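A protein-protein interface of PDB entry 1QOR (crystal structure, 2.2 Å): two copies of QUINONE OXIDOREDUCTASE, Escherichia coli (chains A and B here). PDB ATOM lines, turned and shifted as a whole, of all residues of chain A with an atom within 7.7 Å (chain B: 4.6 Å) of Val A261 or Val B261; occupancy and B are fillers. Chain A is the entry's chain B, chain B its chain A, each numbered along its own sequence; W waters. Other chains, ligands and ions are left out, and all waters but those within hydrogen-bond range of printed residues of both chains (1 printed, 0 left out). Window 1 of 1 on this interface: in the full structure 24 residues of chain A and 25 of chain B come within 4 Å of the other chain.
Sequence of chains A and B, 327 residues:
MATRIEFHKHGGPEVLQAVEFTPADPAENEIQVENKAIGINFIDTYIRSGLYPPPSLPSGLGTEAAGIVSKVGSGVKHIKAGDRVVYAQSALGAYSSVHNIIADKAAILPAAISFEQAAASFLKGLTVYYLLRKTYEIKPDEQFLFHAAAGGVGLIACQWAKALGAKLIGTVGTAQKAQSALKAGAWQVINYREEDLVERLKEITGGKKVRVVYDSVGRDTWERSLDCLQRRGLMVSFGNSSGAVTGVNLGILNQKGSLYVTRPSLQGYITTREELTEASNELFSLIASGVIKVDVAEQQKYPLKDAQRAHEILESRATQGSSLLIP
The backbone NH (N) of Leu B250 sits at hydrogen-bond distance from the backbone carbonyl oxygen (O) of Val A245. The backbone carbonyl oxygen of Leu B259 is in hydrogen-bond range of the side-chain hydroxyl of Thr A262 (2.8 Å). The backbone NH (N) of Val A261 is in hydrogen-bond range of the backbone carbonyl oxygen (O) of Val B261 (2.8 Å). OG1 of Thr B262 is in hydrogen-bond range of O of Leu A259 (2.8 Å).
O of Met B235 is in hydrogen-bond range of N of Thr B262, 3.1 Å away. O of Gly A233 is in hydrogen-bond range of N of Tyr A260 (3.0 Å). The backbone carbonyl oxygen of Met A235 lies within hydrogen-bond range of the backbone NH of Thr A262 (3.0 Å). The backbone carbonyl oxygen (O) of Thr A262 lies within hydrogen-bond range of the backbone NH (N) of Ser A237. O of Leu A253 is in hydrogen-bond range of N of Ser A258 (2.9 Å). The backbone NH of Leu A259 is in hydrogen-bond range of the backbone carbonyl oxygen of Leu A253 (2.8 Å).
Among the printed residues, pairs that only touch across the chains: Trp A222 with Leu B250 (3.7 Å), Ser A237 with Leu B250 (3.7 Å), Leu A250 with Trp B222 (3.5 Å), Leu A250 with Arg B263 (3.5 Å), Leu A253 with Arg B263 (3.8 Å), Ser A258 with Thr B262 (3.8 Å), Ser A258 with Arg B263 (3.8 Å), Leu A259 with Arg B263 (3.6 Å), Tyr A260 with Leu B234 (3.9 Å), Tyr A260 with Val B261 (3.3 Å), Tyr A260 with Thr B262 (3.6 Å), Val A261 with Tyr B260 (3.3 Å), Thr A262 with Tyr B260 (3.6 Å), Arg A263 with Leu B250 (3.4 Å), Arg A263 with Leu B253 (3.8 Å) and Arg A263 with Leu B259 (3.7 Å).
Val B261 touches just these residues of chain A: Tyr A260 (3.3 Å) and Val A261 (2.8 Å). Of the printed residues of chain B, Arg A263 touches Leu B250 (3.4 Å), Leu B253 (3.8 Å) and Leu B259 (3.7 Å). Printed residues of chain A within 4 Å of Trp B222: Leu A250 (3.5 Å). Of the printed residues of chain B, Leu A253 touches Arg B263. Val A236 touches none of the printed residues of chain B. Leu A234 touches none of the printed residues of chain B. The nearest printed residue of chain B that does not touch Val A245 is Leu B253 (8.5 Å).
Of the 10 printed residues of chain B, 9 touch a printed residue of chain A. Of the 19 printed residues of chain A, 11 touch a printed residue of chain B. Among the printed residues, no Asp or Glu carboxylate lies within 4 Å of a Lys or Arg side-chain nitrogen of the other chain.
Trp A222 touches Leu B250, and with the chains exchanged Leu A250 touches Trp B222. Leu A250 touches Arg B263, and with the chains exchanged Arg A263 touches Leu B250. Leu A253 touches Arg B263, and with the chains exchanged Arg A263 touches Leu B253. Val A261 touches its own counterpart, Val B261. Positions printed for both chains: 222, 234, 235, 250, 253, 259, 260, 261, 262 and 263.
Water W1 bridges the side-chain hydroxyl (OG1) of Thr B262 (2.7 Å) and the backbone carbonyl oxygen (O) of Ser A258 (2.8 Å).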
ATOM      1  N   TRP A 222       2.505  35.939  -0.973  1.00  0.00           N
ATOM      2  CA  TRP A 222       1.516  35.172  -1.732  1.00  0.00           C
ATOM      3  C   TRP A 222       1.813  34.974  -3.231  1.00  0.00           C
ATOM      4  O   TRP A 222       2.014  33.834  -3.706  1.00  0.00           O
ATOM      5  CB  TRP A 222       0.113  35.795  -1.494  1.00  0.00           C
ATOM      6  CG  TRP A 222      -1.025  35.218  -2.319  1.00  0.00           C
ATOM      7  CD1 TRP A 222      -1.756  35.886  -3.264  1.00  0.00           C
ATOM      8  CD2 TRP A 222      -1.568  33.877  -2.265  1.00  0.00           C
ATOM      9  NE1 TRP A 222      -2.704  35.057  -3.797  1.00  0.00           N
ATOM     10  CE2 TRP A 222      -2.621  33.819  -3.206  1.00  0.00           C
ATOM     11  CE3 TRP A 222      -1.271  32.722  -1.512  1.00  0.00           C
ATOM     12  CZ2 TRP A 222      -3.393  32.635  -3.422  1.00  0.00           C
ATOM     13  CZ3 TRP A 222      -2.041  31.549  -1.728  1.00  0.00           C
ATOM     14  CH2 TRP A 222      -3.086  31.524  -2.675  1.00  0.00           C
ATOM     15  N   LEU A 226       3.399  31.471  -5.404  1.00  0.00           N
ATOM     16  CA  LEU A 226       2.680  30.835  -6.520  1.00  0.00           C
ATOM     17  C   LEU A 226       3.542  30.770  -7.773  1.00  0.00           C
ATOM     18  O   LEU A 226       3.440  29.827  -8.554  1.00  0.00           O
ATOM     19  CB  LEU A 226       1.393  31.589  -6.837  1.00  0.00           C
ATOM     20  CG  LEU A 226       0.446  31.636  -5.627  1.00  0.00           C
ATOM     21  CD1 LEU A 226      -0.786  32.536  -5.938  1.00  0.00           C
ATOM     22  CD2 LEU A 226       0.037  30.202  -5.212  1.00  0.00           C
ATOM     23  N   LEU A 229       6.014  27.689  -8.240  1.00  0.00           N
ATOM     24  CA  LEU A 229       5.513  26.326  -8.351  1.00  0.00           C
ATOM     25  C   LEU A 229       5.398  25.725  -9.719  1.00  0.00           C
ATOM     26  O   LEU A 229       5.027  26.406 -10.677  1.00  0.00           O
ATOM     27  CB  LEU A 229       4.139  26.204  -7.635  1.00  0.00           C
ATOM     28  CG  LEU A 229       4.117  26.029  -6.099  1.00  0.00           C
ATOM     29  CD1 LEU A 229       2.785  26.408  -5.525  1.00  0.00           C
ATOM     30  CD2 LEU A 229       4.429  24.605  -5.750  1.00  0.00           C
ATOM     31  N   GLY A 233       1.343  22.031  -8.772  1.00  0.00           N
ATOM     32  CA  GLY A 233       2.015  21.922  -7.492  1.00  0.00           C
ATOM     33  C   GLY A 233       1.073  22.358  -6.374  1.00  0.00           C
ATOM     34  O   GLY A 233      -0.043  22.835  -6.610  1.00  0.00           O
ATOM     35  N   LEU A 234       1.554  22.246  -5.147  1.00  0.00           N
ATOM     36  CA  LEU A 234       0.774  22.568  -3.971  1.00  0.00           C
ATOM     37  C   LEU A 234       1.319  23.777  -3.189  1.00  0.00           C
ATOM     38  O   LEU A 234       2.450  23.773  -2.745  1.00  0.00           O
ATOM     39  CB  LEU A 234       0.796  21.333  -3.036  1.00  0.00           C
ATOM     40  CG  LEU A 234       0.126  21.416  -1.664  1.00  0.00           C
ATOM     41  CD1 LEU A 234      -1.363  21.678  -1.813  1.00  0.00           C
ATOM     42  CD2 LEU A 234       0.351  20.153  -0.901  1.00  0.00           C
ATOM     43  N   MET A 235       0.451  24.732  -2.905  1.00  0.00           N
ATOM     44  CA  MET A 235       0.787  25.896  -2.116  1.00  0.00           C
ATOM     45  C   MET A 235       0.189  25.646  -0.724  1.00  0.00           C
ATOM     46  O   MET A 235      -1.031  25.505  -0.579  1.00  0.00           O
ATOM     47  CB  MET A 235       0.144  27.142  -2.732  1.00  0.00           C
ATOM     48  CG  MET A 235       0.161  28.331  -1.787  1.00  0.00           C
ATOM     49  SD  MET A 235       1.874  28.876  -1.448  1.00  0.00           S
ATOM     50  CE  MET A 235       1.513  30.367  -0.543  1.00  0.00           C
ATOM     51  N   VAL A 236       1.048  25.502   0.286  1.00  0.00           N
ATOM     52  CA  VAL A 236       0.586  25.298   1.667  1.00  0.00           C
ATOM     53  C   VAL A 236       0.693  26.611   2.464  1.00  0.00           C
ATOM     54  O   VAL A 236       1.771  26.987   2.920  1.00  0.00           O
ATOM     55  CB  VAL A 236       1.415  24.181   2.391  1.00  0.00           C
ATOM     56  CG1 VAL A 236       0.823  23.885   3.773  1.00  0.00           C
ATOM     57  CG2 VAL A 236       1.509  22.906   1.515  1.00  0.00           C
ATOM     58  N   SER A 237      -0.416  27.330   2.586  1.00  0.00           N
ATOM     59  CA  SER A 237      -0.449  28.588   3.330  1.00  0.00           C
ATOM     60  C   SER A 237      -0.794  28.231   4.784  1.00  0.00           C
ATOM     61  O   SER A 237      -1.966  27.979   5.097  1.00  0.00           O
ATOM     62  CB  SER A 237      -1.522  29.506   2.724  1.00  0.00           C
ATOM     63  OG  SER A 237      -1.718  30.704   3.472  1.00  0.00           O
ATOM     64  N   VAL A 245      -3.863  36.099   4.019  1.00  0.00           N
ATOM     65  CA  VAL A 245      -3.986  36.287   2.587  1.00  0.00           C
ATOM     66  C   VAL A 245      -5.482  36.354   2.237  1.00  0.00           C
ATOM     67  O   VAL A 245      -6.261  35.425   2.482  1.00  0.00           O
ATOM     68  CB  VAL A 245      -3.095  35.346   1.759  1.00  0.00           C
ATOM     69  CG1 VAL A 245      -2.351  34.387   2.626  1.00  0.00           C
ATOM     70  CG2 VAL A 245      -3.819  34.774   0.550  1.00  0.00           C
ATOM     71  N   VAL A 248      -8.382  36.966  -2.521  1.00  0.00           N
ATOM     72  CA  VAL A 248      -7.969  36.153  -3.663  1.00  0.00           C
ATOM     73  C   VAL A 248      -9.111  35.767  -4.656  1.00  0.00           C
ATOM     74  O   VAL A 248     -10.316  35.620  -4.289  1.00  0.00           O
ATOM     75  CB  VAL A 248      -7.042  34.940  -3.233  1.00  0.00           C
ATOM     76  CG1 VAL A 248      -6.720  34.976  -1.725  1.00  0.00           C
ATOM     77  CG2 VAL A 248      -7.570  33.612  -3.699  1.00  0.00           C
ATOM     78  N   LEU A 250      -9.972  33.016  -7.320  1.00  0.00           N
ATOM     79  CA  LEU A 250      -9.505  31.661  -7.643  1.00  0.00           C
ATOM     80  C   LEU A 250      -8.919  31.478  -9.007  1.00  0.00           C
ATOM     81  O   LEU A 250      -8.180  30.532  -9.188  1.00  0.00           O
ATOM     82  CB  LEU A 250     -10.544  30.566  -7.358  1.00  0.00           C
ATOM     83  CG  LEU A 250     -10.973  30.327  -5.898  1.00  0.00           C
ATOM     84  CD1 LEU A 250     -11.806  29.057  -5.935  1.00  0.00           C
ATOM     85  CD2 LEU A 250      -9.790  30.197  -4.883  1.00  0.00           C
ATOM     86  N   LEU A 253      -5.151  30.501  -9.490  1.00  0.00           N
ATOM     87  CA  LEU A 253      -4.617  29.140  -9.388  1.00  0.00           C
ATOM     88  C   LEU A 253      -4.597  28.450 -10.750  1.00  0.00           C
ATOM     89  O   LEU A 253      -3.813  27.530 -10.995  1.00  0.00           O
ATOM     90  CB  LEU A 253      -5.466  28.331  -8.408  1.00  0.00           C
ATOM     91  CG  LEU A 253      -5.623  28.934  -6.989  1.00  0.00           C
ATOM     92  CD1 LEU A 253      -6.492  28.014  -6.099  1.00  0.00           C
ATOM     93  CD2 LEU A 253      -4.203  29.088  -6.392  1.00  0.00           C
ATOM     94  N   SER A 258      -2.800  25.497 -12.765  1.00  0.00           N
ATOM     95  CA  SER A 258      -3.730  24.499 -12.187  1.00  0.00           C
ATOM     96  C   SER A 258      -3.219  24.057 -10.826  1.00  0.00           C
ATOM     97  O   SER A 258      -3.120  22.854 -10.543  1.00  0.00           O
ATOM     98  CB  SER A 258      -3.871  23.276 -13.097  1.00  0.00           C
ATOM     99  OG  SER A 258      -4.657  23.619 -14.237  1.00  0.00           O
ATOM    100  N   LEU A 259      -2.954  25.036  -9.968  1.00  0.00           N
ATOM    101  CA  LEU A 259      -2.377  24.735  -8.678  1.00  0.00           C
ATOM    102  C   LEU A 259      -3.397  24.323  -7.654  1.00  0.00           C
ATOM    103  O   LEU A 259      -4.595  24.576  -7.799  1.00  0.00           O
ATOM    104  CB  LEU A 259      -1.604  25.970  -8.174  1.00  0.00           C
ATOM    105  CG  LEU A 259      -0.480  26.619  -9.038  1.00  0.00           C
ATOM    106  CD1 LEU A 259       0.107  27.886  -8.289  1.00  0.00           C
ATOM    107  CD2 LEU A 259       0.649  25.595  -9.333  1.00  0.00           C
ATOM    108  N   TYR A 260      -2.877  23.735  -6.586  1.00  0.00           N
ATOM    109  CA  TYR A 260      -3.661  23.332  -5.422  1.00  0.00           C
ATOM    110  C   TYR A 260      -3.207  24.233  -4.286  1.00  0.00           C
ATOM    111  O   TYR A 260      -2.034  24.585  -4.217  1.00  0.00           O
ATOM    112  CB  TYR A 260      -3.306  21.903  -4.994  1.00  0.00           C
ATOM    113  CG  TYR A 260      -3.825  20.808  -5.887  1.00  0.00           C
ATOM    114  CD1 TYR A 260      -3.149  20.467  -7.057  1.00  0.00           C
ATOM    115  CD2 TYR A 260      -4.953  20.039  -5.509  1.00  0.00           C
ATOM    116  CE1 TYR A 260      -3.552  19.377  -7.830  1.00  0.00           C
ATOM    117  CE2 TYR A 260      -5.378  18.943  -6.283  1.00  0.00           C
ATOM    118  CZ  TYR A 260      -4.664  18.617  -7.431  1.00  0.00           C
ATOM    119  OH  TYR A 260      -5.003  17.521  -8.173  1.00  0.00           O
ATOM    120  N   VAL A 261      -4.110  24.592  -3.394  1.00  0.00           N
ATOM    121  CA  VAL A 261      -3.735  25.360  -2.251  1.00  0.00           C
ATOM    122  C   VAL A 261      -4.485  24.793  -1.038  1.00  0.00           C
ATOM    123  O   VAL A 261      -5.578  24.226  -1.167  1.00  0.00           O
ATOM    124  CB  VAL A 261      -4.032  26.875  -2.438  1.00  0.00           C
ATOM    125  CG1 VAL A 261      -5.511  27.131  -2.537  1.00  0.00           C
ATOM    126  CG2 VAL A 261      -3.541  27.630  -1.236  1.00  0.00           C
ATOM    127  N   THR A 262      -3.854  24.837   0.128  1.00  0.00           N
ATOM    128  CA  THR A 262      -4.522  24.402   1.347  1.00  0.00           C
ATOM    129  C   THR A 262      -4.119  25.340   2.472  1.00  0.00           C
ATOM    130  O   THR A 262      -3.045  25.948   2.427  1.00  0.00           O
ATOM    131  CB  THR A 262      -4.158  22.916   1.737  1.00  0.00           C
ATOM    132  OG1 THR A 262      -4.934  22.506   2.883  1.00  0.00           O
ATOM    133  CG2 THR A 262      -2.645  22.756   1.990  1.00  0.00           C
ATOM    134  N   ARG A 263      -5.009  25.510   3.436  1.00  0.00           N
ATOM    135  CA  ARG A 263      -4.708  26.352   4.593  1.00  0.00           C
ATOM    136  C   ARG A 263      -4.978  25.467   5.825  1.00  0.00           C
ATOM    137  O   ARG A 263      -6.039  25.508   6.426  1.00  0.00           O
ATOM    138  CB  ARG A 263      -5.583  27.606   4.594  1.00  0.00           C
ATOM    139  CG  ARG A 263      -4.915  28.807   5.297  1.00  0.00           C
ATOM    140  CD  ARG A 263      -4.387  28.427   6.672  1.00  0.00           C
ATOM    141  NE  ARG A 263      -3.864  29.613   7.357  1.00  0.00           N
ATOM    142  CZ  ARG A 263      -3.341  29.621   8.570  1.00  0.00           C
ATOM    143  NH1 ARG A 263      -3.261  28.480   9.266  1.00  0.00           N
ATOM    144  NH2 ARG A 263      -2.891  30.772   9.067  1.00  0.00           N
ATOM    145  N   PRO A 264      -3.981  24.705   6.246  1.00  0.00           N
ATOM    146  CA  PRO A 264      -4.184  23.826   7.388  1.00  0.00           C
ATOM    147  C   PRO A 264      -3.907  24.422   8.760  1.00  0.00           C
ATOM    148  O   PRO A 264      -3.288  25.488   8.879  1.00  0.00           O
ATOM    149  CB  PRO A 264      -3.207  22.697   7.076  1.00  0.00           C
ATOM    150  CG  PRO A 264      -2.003  23.484   6.556  1.00  0.00           C
ATOM    151  CD  PRO A 264      -2.617  24.571   5.694  1.00  0.00           C
ATOM    152  N   TRP B 222     -20.142  28.451  -3.817  1.00  0.00           N
ATOM    153  CA  TRP B 222     -18.888  28.424  -3.090  1.00  0.00           C
ATOM    154  C   TRP B 222     -18.976  28.010  -1.616  1.00  0.00           C
ATOM    155  O   TRP B 222     -18.347  27.045  -1.184  1.00  0.00           O
ATOM    156  CB  TRP B 222     -18.173  29.802  -3.249  1.00  0.00           C
ATOM    157  CG  TRP B 222     -16.862  29.947  -2.445  1.00  0.00           C
ATOM    158  CD1 TRP B 222     -16.655  30.770  -1.380  1.00  0.00           C
ATOM    159  CD2 TRP B 222     -15.630  29.195  -2.620  1.00  0.00           C
ATOM    160  NE1 TRP B 222     -15.393  30.575  -0.883  1.00  0.00           N
ATOM    161  CE2 TRP B 222     -14.741  29.619  -1.619  1.00  0.00           C
ATOM    162  CE3 TRP B 222     -15.202  28.219  -3.535  1.00  0.00           C
ATOM    163  CZ2 TRP B 222     -13.437  29.102  -1.492  1.00  0.00           C
ATOM    164  CZ3 TRP B 222     -13.894  27.708  -3.417  1.00  0.00           C
ATOM    165  CH2 TRP B 222     -13.030  28.154  -2.397  1.00  0.00           C
ATOM    166  N   LEU B 234     -11.235  17.838  -0.637  1.00  0.00           N
ATOM    167  CA  LEU B 234     -10.780  18.609  -1.784  1.00  0.00           C
ATOM    168  C   LEU B 234     -11.884  19.286  -2.534  1.00  0.00           C
ATOM    169  O   LEU B 234     -12.795  18.616  -3.003  1.00  0.00           O
ATOM    170  CB  LEU B 234     -10.033  17.716  -2.753  1.00  0.00           C
ATOM    171  CG  LEU B 234      -9.585  18.365  -4.076  1.00  0.00           C
ATOM    172  CD1 LEU B 234      -8.420  19.403  -3.926  1.00  0.00           C
ATOM    173  CD2 LEU B 234      -9.158  17.224  -4.999  1.00  0.00           C
ATOM    174  N   MET B 235     -11.795  20.610  -2.664  1.00  0.00           N
ATOM    175  CA  MET B 235     -12.778  21.396  -3.392  1.00  0.00           C
ATOM    176  C   MET B 235     -12.191  21.682  -4.784  1.00  0.00           C
ATOM    177  O   MET B 235     -11.093  22.273  -4.883  1.00  0.00           O
ATOM    178  CB  MET B 235     -13.084  22.699  -2.624  1.00  0.00           C
ATOM    179  CG  MET B 235     -13.791  23.782  -3.432  1.00  0.00           C
ATOM    180  SD  MET B 235     -15.457  23.319  -3.964  1.00  0.00           S
ATOM    181  CE  MET B 235     -16.265  24.889  -4.386  1.00  0.00           C
ATOM    182  N   LEU B 250      -8.216  33.090   2.707  1.00  0.00           N
ATOM    183  CA  LEU B 250      -7.778  31.724   2.867  1.00  0.00           C
ATOM    184  C   LEU B 250      -8.109  31.131   4.221  1.00  0.00           C
ATOM    185  O   LEU B 250      -8.112  29.910   4.370  1.00  0.00           O
ATOM    186  CB  LEU B 250      -6.272  31.590   2.611  1.00  0.00           C
ATOM    187  CG  LEU B 250      -5.796  31.691   1.165  1.00  0.00           C
ATOM    188  CD1 LEU B 250      -4.460  30.978   1.064  1.00  0.00           C
ATOM    189  CD2 LEU B 250      -6.786  31.031   0.213  1.00  0.00           C
ATOM    190  N   LEU B 253     -10.518  28.207   4.466  1.00  0.00           N
ATOM    191  CA  LEU B 253     -10.160  26.802   4.238  1.00  0.00           C
ATOM    192  C   LEU B 253      -9.763  26.117   5.568  1.00  0.00           C
ATOM    193  O   LEU B 253      -9.828  24.866   5.754  1.00  0.00           O
ATOM    194  CB  LEU B 253      -9.005  26.700   3.235  1.00  0.00           C
ATOM    195  CG  LEU B 253      -9.301  27.370   1.899  1.00  0.00           C
ATOM    196  CD1 LEU B 253      -8.107  27.254   0.860  1.00  0.00           C
ATOM    197  CD2 LEU B 253     -10.600  26.684   1.374  1.00  0.00           C
ATOM    198  N   LEU B 259      -9.145  22.363   4.460  1.00  0.00           N
ATOM    199  CA  LEU B 259      -9.491  21.879   3.141  1.00  0.00           C
ATOM    200  C   LEU B 259      -8.447  22.253   2.092  1.00  0.00           C
ATOM    201  O   LEU B 259      -7.584  23.119   2.332  1.00  0.00           O
ATOM    202  CB  LEU B 259     -10.820  22.523   2.738  1.00  0.00           C
ATOM    203  CG  LEU B 259     -12.018  22.353   3.696  1.00  0.00           C
ATOM    204  CD1 LEU B 259     -13.258  23.092   3.185  1.00  0.00           C
ATOM    205  CD2 LEU B 259     -12.305  20.856   3.835  1.00  0.00           C
ATOM    206  N   TYR B 260      -8.484  21.515   0.975  1.00  0.00           N
ATOM    207  CA  TYR B 260      -7.659  21.798  -0.186  1.00  0.00           C
ATOM    208  C   TYR B 260      -8.605  22.340  -1.281  1.00  0.00           C
ATOM    209  O   TYR B 260      -9.815  22.059  -1.295  1.00  0.00           O
ATOM    210  CB  TYR B 260      -6.980  20.579  -0.739  1.00  0.00           C
ATOM    211  CG  TYR B 260      -5.950  19.924   0.139  1.00  0.00           C
ATOM    212  CD1 TYR B 260      -6.324  19.191   1.268  1.00  0.00           C
ATOM    213  CD2 TYR B 260      -4.600  19.902  -0.236  1.00  0.00           C
ATOM    214  CE1 TYR B 260      -5.392  18.447   1.979  1.00  0.00           C
ATOM    215  CE2 TYR B 260      -3.654  19.154   0.483  1.00  0.00           C
ATOM    216  CZ  TYR B 260      -4.068  18.443   1.569  1.00  0.00           C
ATOM    217  OH  TYR B 260      -3.156  17.714   2.246  1.00  0.00           O
ATOM    218  N   VAL B 261      -8.083  23.233  -2.113  1.00  0.00           N
ATOM    219  CA  VAL B 261      -8.836  23.739  -3.242  1.00  0.00           C
ATOM    220  C   VAL B 261      -7.887  23.851  -4.445  1.00  0.00           C
ATOM    221  O   VAL B 261      -6.681  24.111  -4.293  1.00  0.00           O
ATOM    222  CB  VAL B 261      -9.611  25.043  -2.918  1.00  0.00           C
ATOM    223  CG1 VAL B 261      -8.695  26.076  -2.401  1.00  0.00           C
ATOM    224  CG2 VAL B 261     -10.312  25.580  -4.187  1.00  0.00           C
ATOM    225  N   THR B 262      -8.413  23.572  -5.632  1.00  0.00           N
ATOM    226  CA  THR B 262      -7.617  23.651  -6.839  1.00  0.00           C
ATOM    227  C   THR B 262      -8.549  24.217  -7.868  1.00  0.00           C
ATOM    228  O   THR B 262      -9.769  24.113  -7.707  1.00  0.00           O
ATOM    229  CB  THR B 262      -7.074  22.285  -7.292  1.00  0.00           C
ATOM    230  OG1 THR B 262      -6.267  22.457  -8.473  1.00  0.00           O
ATOM    231  CG2 THR B 262      -8.232  21.291  -7.588  1.00  0.00           C
ATOM    232  N   ARG B 263      -7.991  24.989  -8.807  1.00  0.00           N
ATOM    233  CA  ARG B 263      -8.792  25.592  -9.870  1.00  0.00           C
ATOM    234  C   ARG B 263      -8.090  25.167 -11.166  1.00  0.00           C
ATOM    235  O   ARG B 263      -7.237  25.876 -11.685  1.00  0.00           O
ATOM    236  CB  ARG B 263      -8.838  27.106  -9.716  1.00  0.00           C
ATOM    237  CG  ARG B 263     -10.075  27.744 -10.339  1.00  0.00           C
ATOM    238  CD  ARG B 263     -10.301  27.313 -11.819  1.00  0.00           C
ATOM    239  NE  ARG B 263     -11.525  27.895 -12.379  1.00  0.00           N
ATOM    240  CZ  ARG B 263     -11.987  27.639 -13.600  1.00  0.00           C
ATOM    241  NH1 ARG B 263     -11.344  26.795 -14.408  1.00  0.00           N
ATOM    242  NH2 ARG B 263     -13.069  28.272 -14.031  1.00  0.00           N
HETATM  243  O   HOH W   1      -5.267  21.039 -10.498  1.00  0.00           O
